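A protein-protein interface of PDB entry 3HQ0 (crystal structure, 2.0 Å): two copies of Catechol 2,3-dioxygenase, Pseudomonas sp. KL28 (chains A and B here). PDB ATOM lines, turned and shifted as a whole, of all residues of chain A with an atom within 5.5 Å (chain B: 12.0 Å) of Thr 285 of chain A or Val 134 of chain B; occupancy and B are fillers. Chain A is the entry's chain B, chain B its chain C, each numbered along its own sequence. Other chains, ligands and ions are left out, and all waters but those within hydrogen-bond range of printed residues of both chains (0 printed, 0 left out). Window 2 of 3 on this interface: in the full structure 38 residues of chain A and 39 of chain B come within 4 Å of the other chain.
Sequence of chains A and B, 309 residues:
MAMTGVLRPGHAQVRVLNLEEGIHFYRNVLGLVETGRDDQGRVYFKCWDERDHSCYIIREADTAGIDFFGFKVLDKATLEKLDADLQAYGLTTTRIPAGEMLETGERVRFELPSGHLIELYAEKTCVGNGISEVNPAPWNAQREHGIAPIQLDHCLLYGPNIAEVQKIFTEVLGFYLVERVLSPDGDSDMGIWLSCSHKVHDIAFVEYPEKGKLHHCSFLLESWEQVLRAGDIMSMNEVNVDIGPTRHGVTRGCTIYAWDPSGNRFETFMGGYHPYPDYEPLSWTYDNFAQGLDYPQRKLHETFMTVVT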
ATOM      1  N   VAL A 181       9.584  16.329 -23.560  1.00  0.00           N
ATOM      2  CA  VAL A 181       8.585  16.275 -24.611  1.00  0.00           C
ATOM      3  C   VAL A 181       7.599  15.207 -24.168  1.00  0.00           C
ATOM      4  O   VAL A 181       8.002  14.123 -23.766  1.00  0.00           O
ATOM      5  CB  VAL A 181       9.198  15.851 -25.956  1.00  0.00           C
ATOM      6  CG1 VAL A 181       8.096  15.458 -26.919  1.00  0.00           C
ATOM      7  CG2 VAL A 181      10.027  16.983 -26.533  1.00  0.00           C
ATOM      8  N   LEU A 182       6.311  15.509 -24.230  1.00  0.00           N
ATOM      9  CA  LEU A 182       5.310  14.538 -23.816  1.00  0.00           C
ATOM     10  C   LEU A 182       4.935  13.624 -24.970  1.00  0.00           C
ATOM     11  O   LEU A 182       5.076  13.987 -26.141  1.00  0.00           O
ATOM     12  CB  LEU A 182       4.062  15.251 -23.289  1.00  0.00           C
ATOM     13  CG  LEU A 182       4.218  16.036 -21.984  1.00  0.00           C
ATOM     14  CD1 LEU A 182       5.136  17.223 -22.198  1.00  0.00           C
ATOM     15  CD2 LEU A 182       2.856  16.509 -21.514  1.00  0.00           C
ATOM     16  N   SER A 283       7.712  21.896 -20.430  1.00  0.00           N
ATOM     17  CA  SER A 283       7.251  20.743 -21.193  1.00  0.00           C
ATOM     18  C   SER A 283       6.773  21.101 -22.590  1.00  0.00           C
ATOM     19  O   SER A 283       6.361  22.232 -22.849  1.00  0.00           O
ATOM     20  CB  SER A 283       6.133  20.032 -20.423  1.00  0.00           C
ATOM     21  OG  SER A 283       5.071  20.927 -20.161  1.00  0.00           O
ATOM     22  N   TRP A 284       6.845  20.123 -23.487  1.00  0.00           N
ATOM     23  CA  TRP A 284       6.412  20.303 -24.865  1.00  0.00           C
ATOM     24  C   TRP A 284       5.468  19.166 -25.262  1.00  0.00           C
ATOM     25  O   TRP A 284       5.771  17.992 -25.045  1.00  0.00           O
ATOM     26  CB  TRP A 284       7.607  20.307 -25.819  1.00  0.00           C
ATOM     27  CG  TRP A 284       8.620  21.370 -25.536  1.00  0.00           C
ATOM     28  CD1 TRP A 284       9.646  21.304 -24.641  1.00  0.00           C
ATOM     29  CD2 TRP A 284       8.696  22.664 -26.141  1.00  0.00           C
ATOM     30  NE1 TRP A 284      10.360  22.477 -24.650  1.00  0.00           N
ATOM     31  CE2 TRP A 284       9.798  23.331 -25.562  1.00  0.00           C
ATOM     32  CE3 TRP A 284       7.942  23.328 -27.116  1.00  0.00           C
ATOM     33  CZ2 TRP A 284      10.163  24.632 -25.924  1.00  0.00           C
ATOM     34  CZ3 TRP A 284       8.305  24.625 -27.477  1.00  0.00           C
ATOM     35  CH2 TRP A 284       9.405  25.260 -26.881  1.00  0.00           C
ATOM     36  N   THR A 285       4.330  19.511 -25.843  1.00  0.00           N
ATOM     37  CA  THR A 285       3.372  18.496 -26.262  1.00  0.00           C
ATOM     38  C   THR A 285       3.912  17.784 -27.482  1.00  0.00           C
ATOM     39  O   THR A 285       4.601  18.389 -28.300  1.00  0.00           O
ATOM     40  CB  THR A 285       2.019  19.117 -26.605  1.00  0.00           C
ATOM     41  OG1 THR A 285       2.206  20.149 -27.577  1.00  0.00           O
ATOM     42  CG2 THR A 285       1.374  19.695 -25.361  1.00  0.00           C
ATOM     43  N   TYR A 286       3.600  16.497 -27.599  1.00  0.00           N
ATOM     44  CA  TYR A 286       4.067  15.688 -28.716  1.00  0.00           C
ATOM     45  C   TYR A 286       3.870  16.381 -30.053  1.00  0.00           C
ATOM     46  O   TYR A 286       4.777  16.415 -30.882  1.00  0.00           O
ATOM     47  CB  TYR A 286       3.343  14.344 -28.758  1.00  0.00           C
ATOM     48  CG  TYR A 286       3.973  13.356 -29.720  1.00  0.00           C
ATOM     49  CD1 TYR A 286       5.194  12.743 -29.420  1.00  0.00           C
ATOM     50  CD2 TYR A 286       3.360  13.040 -30.938  1.00  0.00           C
ATOM     51  CE1 TYR A 286       5.788  11.838 -30.302  1.00  0.00           C
ATOM     52  CE2 TYR A 286       3.949  12.136 -31.830  1.00  0.00           C
ATOM     53  CZ  TYR A 286       5.162  11.540 -31.502  1.00  0.00           C
ATOM     54  OH  TYR A 286       5.750  10.638 -32.366  1.00  0.00           O
ATOM     55  N   ASP A 287       2.678  16.924 -30.268  1.00  0.00           N
ATOM     56  CA  ASP A 287       2.387  17.595 -31.528  1.00  0.00           C
ATOM     57  C   ASP A 287       3.417  18.673 -31.858  1.00  0.00           C
ATOM     58  O   ASP A 287       3.741  18.895 -33.024  1.00  0.00           O
ATOM     59  CB  ASP A 287       0.970  18.184 -31.505  1.00  0.00           C
ATOM     60  CG  ASP A 287       0.709  19.038 -30.282  1.00  0.00           C
ATOM     61  OD1 ASP A 287       1.414  20.057 -30.106  1.00  0.00           O
ATOM     62  OD2 ASP A 287      -0.208  18.693 -29.499  1.00  0.00           O
ATOM     63  N   ASN A 288       3.945  19.334 -30.835  1.00  0.00           N
ATOM     64  CA  ASN A 288       4.945  20.369 -31.058  1.00  0.00           C
ATOM     65  C   ASN A 288       6.273  19.694 -31.403  1.00  0.00           C
ATOM     66  O   ASN A 288       7.005  20.142 -32.289  1.00  0.00           O
ATOM     67  CB  ASN A 288       5.111  21.225 -29.807  1.00  0.00           C
ATOM     68  CG  ASN A 288       5.516  22.646 -30.131  1.00  0.00           C
ATOM     69  OD1 ASN A 288       4.691  23.453 -30.572  1.00  0.00           O
ATOM     70  ND2 ASN A 288       6.793  22.962 -29.927  1.00  0.00           N
ATOM     71  N   PHE A 289       6.573  18.608 -30.700  1.00  0.00           N
ATOM     72  CA  PHE A 289       7.800  17.861 -30.940  1.00  0.00           C
ATOM     73  C   PHE A 289       7.749  17.214 -32.320  1.00  0.00           C
ATOM     74  O   PHE A 289       6.624  17.003 -32.836  1.00  0.00           O
ATOM     75  CB  PHE A 289       7.968  16.776 -29.877  1.00  0.00           C
ATOM     76  CG  PHE A 289       9.230  15.963 -30.021  1.00  0.00           C
ATOM     77  CD1 PHE A 289      10.481  16.572 -29.955  1.00  0.00           C
ATOM     78  CD2 PHE A 289       9.165  14.581 -30.189  1.00  0.00           C
ATOM     79  CE1 PHE A 289      11.651  15.815 -30.049  1.00  0.00           C
ATOM     80  CE2 PHE A 289      10.329  13.814 -30.285  1.00  0.00           C
ATOM     81  CZ  PHE A 289      11.574  14.433 -30.214  1.00  0.00           C
ATOM     82  N   ARG B  51      12.747  33.504 -12.439  1.00  0.00           N
ATOM     83  CA  ARG B  51      11.493  32.892 -12.033  1.00  0.00           C
ATOM     84  C   ARG B  51      11.016  33.265 -10.638  1.00  0.00           C
ATOM     85  O   ARG B  51       9.816  33.204 -10.348  1.00  0.00           O
ATOM     86  CB  ARG B  51      11.614  31.374 -12.154  1.00  0.00           C
ATOM     87  CG  ARG B  51      11.925  30.930 -13.570  1.00  0.00           C
ATOM     88  CD  ARG B  51      11.743  29.445 -13.744  1.00  0.00           C
ATOM     89  NE  ARG B  51      12.196  29.009 -15.058  1.00  0.00           N
ATOM     90  CZ  ARG B  51      12.167  27.751 -15.472  1.00  0.00           C
ATOM     91  NH1 ARG B  51      11.697  26.804 -14.673  1.00  0.00           N
ATOM     92  NH2 ARG B  51      12.621  27.437 -16.675  1.00  0.00           N
ATOM     93  N   VAL B 127       7.357  32.909  -9.298  1.00  0.00           N
ATOM     94  CA  VAL B 127       6.279  33.505 -10.071  1.00  0.00           C
ATOM     95  C   VAL B 127       6.392  33.211 -11.566  1.00  0.00           C
ATOM     96  O   VAL B 127       5.456  33.462 -12.328  1.00  0.00           O
ATOM     97  CB  VAL B 127       6.246  35.022  -9.869  1.00  0.00           C
ATOM     98  CG1 VAL B 127       4.957  35.591 -10.437  1.00  0.00           C
ATOM     99  CG2 VAL B 127       6.370  35.346  -8.382  1.00  0.00           C
ATOM    100  N   GLY B 128       7.537  32.685 -11.987  1.00  0.00           N
ATOM    101  CA  GLY B 128       7.723  32.367 -13.392  1.00  0.00           C
ATOM    102  C   GLY B 128       8.243  33.539 -14.200  1.00  0.00           C
ATOM    103  O   GLY B 128       8.351  34.654 -13.688  1.00  0.00           O
ATOM    104  N   ASN B 129       8.553  33.286 -15.470  1.00  0.00           N
ATOM    105  CA  ASN B 129       9.081  34.315 -16.360  1.00  0.00           C
ATOM    106  C   ASN B 129       8.030  34.941 -17.279  1.00  0.00           C
ATOM    107  O   ASN B 129       8.365  35.506 -18.319  1.00  0.00           O
ATOM    108  CB  ASN B 129      10.217  33.735 -17.215  1.00  0.00           C
ATOM    109  CG  ASN B 129       9.746  32.637 -18.155  1.00  0.00           C
ATOM    110  OD1 ASN B 129      10.476  32.233 -19.064  1.00  0.00           O
ATOM    111  ND2 ASN B 129       8.532  32.144 -17.939  1.00  0.00           N
ATOM    112  N   GLY B 130       6.761  34.833 -16.904  1.00  0.00           N
ATOM    113  CA  GLY B 130       5.710  35.419 -17.714  1.00  0.00           C
ATOM    114  C   GLY B 130       5.417  34.683 -19.007  1.00  0.00           C
ATOM    115  O   GLY B 130       4.571  35.117 -19.788  1.00  0.00           O
ATOM    116  N   ILE B 131       6.117  33.579 -19.242  1.00  0.00           N
ATOM    117  CA  ILE B 131       5.905  32.784 -20.440  1.00  0.00           C
ATOM    118  C   ILE B 131       5.326  31.444 -20.016  1.00  0.00           C
ATOM    119  O   ILE B 131       5.583  30.981 -18.906  1.00  0.00           O
ATOM    120  CB  ILE B 131       7.217  32.557 -21.206  1.00  0.00           C
ATOM    121  CG1 ILE B 131       7.867  33.908 -21.516  1.00  0.00           C
ATOM    122  CG2 ILE B 131       6.933  31.794 -22.499  1.00  0.00           C
ATOM    123  CD1 ILE B 131       9.135  33.821 -22.352  1.00  0.00           C
ATOM    124  N   SER B 132       4.549  30.825 -20.896  1.00  0.00           N
ATOM    125  CA  SER B 132       3.916  29.548 -20.584  1.00  0.00           C
ATOM    126  C   SER B 132       4.885  28.431 -20.228  1.00  0.00           C
ATOM    127  O   SER B 132       6.033  28.402 -20.689  1.00  0.00           O
ATOM    128  CB  SER B 132       3.042  29.090 -21.748  1.00  0.00           C
ATOM    129  OG  SER B 132       2.370  27.889 -21.416  1.00  0.00           O
ATOM    130  N   GLU B 133       4.401  27.504 -19.406  1.00  0.00           N
ATOM    131  CA  GLU B 133       5.190  26.358 -18.976  1.00  0.00           C
ATOM    132  C   GLU B 133       5.043  25.230 -19.991  1.00  0.00           C
ATOM    133  O   GLU B 133       5.796  24.257 -19.973  1.00  0.00           O
ATOM    134  CB  GLU B 133       4.720  25.888 -17.600  1.00  0.00           C
ATOM    135  CG  GLU B 133       4.702  26.992 -16.553  1.00  0.00           C
ATOM    136  CD  GLU B 133       4.198  26.508 -15.212  1.00  0.00           C
ATOM    137  OE1 GLU B 133       3.327  25.617 -15.208  1.00  0.00           O
ATOM    138  OE2 GLU B 133       4.657  27.023 -14.171  1.00  0.00           O
ATOM    139  N   VAL B 134       4.067  25.359 -20.881  1.00  0.00           N
ATOM    140  CA  VAL B 134       3.852  24.350 -21.905  1.00  0.00           C
ATOM    141  C   VAL B 134       4.052  25.002 -23.270  1.00  0.00           C
ATOM    142  O   VAL B 134       3.471  26.050 -23.553  1.00  0.00           O
ATOM    143  CB  VAL B 134       2.434  23.747 -21.799  1.00  0.00           C
ATOM    144  CG1 VAL B 134       1.390  24.834 -21.976  1.00  0.00           C
ATOM    145  CG2 VAL B 134       2.260  22.641 -22.826  1.00  0.00           C
ATOM    146  N   ASN B 135       4.893  24.393 -24.102  1.00  0.00           N
ATOM    147  CA  ASN B 135       5.180  24.928 -25.429  1.00  0.00           C
ATOM    148  C   ASN B 135       5.456  26.425 -25.340  1.00  0.00           C
ATOM    149  O   ASN B 135       4.748  27.230 -25.940  1.00  0.00           O
ATOM    150  CB  ASN B 135       3.999  24.688 -26.367  1.00  0.00           C
ATOM    151  CG  ASN B 135       3.646  23.228 -26.488  1.00  0.00           C
ATOM    152  OD1 ASN B 135       4.523  22.373 -26.604  1.00  0.00           O
ATOM    153  ND2 ASN B 135       2.358  22.932 -26.477  1.00  0.00           N
ATOM    154  N   PRO B 136       6.495  26.816 -24.586  1.00  0.00           N
ATOM    155  CA  PRO B 136       6.859  28.223 -24.413  1.00  0.00           C
ATOM    156  C   PRO B 136       7.421  28.901 -25.661  1.00  0.00           C
ATOM    157  O   PRO B 136       8.107  28.277 -26.468  1.00  0.00           O
ATOM    158  CB  PRO B 136       7.885  28.167 -23.288  1.00  0.00           C
ATOM    159  CG  PRO B 136       8.593  26.880 -23.583  1.00  0.00           C
ATOM    160  CD  PRO B 136       7.447  25.941 -23.874  1.00  0.00           C
ATOM    161  N   ALA B 137       7.121  30.185 -25.813  1.00  0.00           N
ATOM    162  CA  ALA B 137       7.634  30.954 -26.939  1.00  0.00           C
ATOM    163  C   ALA B 137       9.101  31.226 -26.623  1.00  0.00           C
ATOM    164  O   ALA B 137       9.549  31.016 -25.491  1.00  0.00           O
ATOM    165  CB  ALA B 137       6.874  32.262 -27.068  1.00  0.00           C
ATOM    166  N   PRO B 138       9.881  31.670 -27.617  1.00  0.00           N
ATOM    167  CA  PRO B 138      11.298  31.946 -27.346  1.00  0.00           C
ATOM    168  C   PRO B 138      11.451  33.112 -26.363  1.00  0.00           C
ATOM    169  O   PRO B 138      12.323  33.114 -25.490  1.00  0.00           O
ATOM    170  CB  PRO B 138      11.851  32.277 -28.732  1.00  0.00           C
ATOM    171  CG  PRO B 138      10.653  32.899 -29.421  1.00  0.00           C
ATOM    172  CD  PRO B 138       9.547  31.949 -29.026  1.00  0.00           C
ATOM    173  N   TRP B 139      10.582  34.103 -26.526  1.00  0.00           N
ATOM    174  CA  TRP B 139      10.569  35.292 -25.686  1.00  0.00           C
ATOM    175  C   TRP B 139       9.263  36.036 -25.948  1.00  0.00           C
ATOM    176  O   TRP B 139       8.462  35.635 -26.802  1.00  0.00           O
ATOM    177  CB  TRP B 139      11.756  36.201 -26.015  1.00  0.00           C
ATOM    178  CG  TRP B 139      11.879  36.506 -27.477  1.00  0.00           C
ATOM    179  CD1 TRP B 139      12.668  35.861 -28.383  1.00  0.00           C
ATOM    180  CD2 TRP B 139      11.150  37.501 -28.216  1.00  0.00           C
ATOM    181  NE1 TRP B 139      12.478  36.388 -29.638  1.00  0.00           N
ATOM    182  CE2 TRP B 139      11.550  37.395 -29.565  1.00  0.00           C
ATOM    183  CE3 TRP B 139      10.195  38.467 -27.869  1.00  0.00           C
ATOM    184  CZ2 TRP B 139      11.029  38.222 -30.569  1.00  0.00           C
ATOM    185  CZ3 TRP B 139       9.677  39.291 -28.876  1.00  0.00           C
ATOM    186  CH2 TRP B 139      10.097  39.160 -30.202  1.00  0.00           C
ATOM    187  N   ASN B 140       9.052  37.126 -25.225  1.00  0.00           N
ATOM    188  CA  ASN B 140       7.830  37.892 -25.393  1.00  0.00           C
ATOM    189  C   ASN B 140       8.104  39.389 -25.402  1.00  0.00           C
ATOM    190  O   ASN B 140       9.250  39.821 -25.500  1.00  0.00           O
ATOM    191  CB  ASN B 140       6.866  37.552 -24.269  1.00  0.00           C
ATOM    192  CG  ASN B 140       7.491  37.732 -22.909  1.00  0.00           C
ATOM    193  OD1 ASN B 140       8.084  38.769 -22.626  1.00  0.00           O
ATOM    194  ND2 ASN B 140       7.363  36.724 -22.058  1.00  0.00           N
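The side-chain hydroxyl (OG) of Ser 132 of chain B is in hydrogen-bond range of the backbone carbonyl oxygen (O) of Val 134 of chain B, at 3.0 Å. O of Trp 284 of chain A lies within hydrogen-bond range of N of Leu 182 of chain A, 2.7 Å away. OG1 of Thr 285 of chain A sits at hydrogen-bond distance from OD1 of Asp 287 of chain A (2.7 Å).
Printed residues of chain B within 4 Å of Ser 283 of chain A: Glu 133 (3.1 Å), Val 134 (3.4 Å), Asn 135 (2.9 Å) and Pro 136 (3.998 Å). Of the printed residues of chain B, Trp 284 of chain A touches Asn 135 and Pro 136. Of the printed residues of chain B, Thr 285 of chain A touches Val 134 and Asn 135. Ile 131 of chain B touches none of the printed residues of chain A. Printed residues of chain A within 4 Å of Glu 133 of chain B: Ser 283 (3.1 Å). Of the printed residues of chain A, Asn 135 of chain B touches Ser 283 (2.9 Å), Trp 284 (3.3 Å), Thr 285 (3.0 Å) and Asn 288 (3.5 Å). Of the printed residues of chain A, Pro 136 of chain B touches Ser 283 and Trp 284. The nearest printed residue of chain B that does not touch Thr 285 of chain A is Pro 136 of chain B (7.4 Å).
Of the 15 printed residues of chain B, 4 touch a printed residue of chain A. Printed residues of chain B that touch a printed residue of chain A: Glu 133, Val 134, Asn 135 and Pro 136. Hydrophobic or aromatic side chains of chain B within 4 Å of the printed part of chain A: Val 134 and Pro 136. Of the 9 printed residues of chain A, 4 touch a printed residue of chain B. Hydrophobic or aromatic side chains of chain A within 4 Å of the printed part of chain B: Trp 284. Among the printed residues, 9 pairs touch across the chains. Among the printed residues, no Asp or Glu carboxylate lies within 4 Å of a Lys or Arg side-chain nitrogen of the other chain.
Ser 283 of chain A touches Val 134 of chain B. O of Ser 283 of chain A touches CD of Pro 136 of chain B, at 3.998 Å. CA of Trp 284 of chain A touches OD1 of Asn 135 of chain B, 3.3 Å away. Pro 136 of chain B touches Trp 284 of chain A. Thr 285 of chain A touches Val 134 of chain B (CG2 to CG2, 3.99 Å). Asn 288 of chain A touches Asn 135 of chain B.
No position is printed for both chains. Of the 9 pairs that touch across the chains among the printed residues, none has its exchanged pair printed and touching as well.
O of Ser 283 of chain A lies within hydrogen-bond range of N of Asn 135 of chain B, at 2.9 Å. The backbone NH (N) of Thr 285 of chain A sits at hydrogen-bond distance from the side-chain amide oxygen (OD1) of Asn 135 of chain B, at 3.0 Å. N of Ser 283 of chain A is in hydrogen-bond range of O of Glu 133 of chain B, 3.1 Å away.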
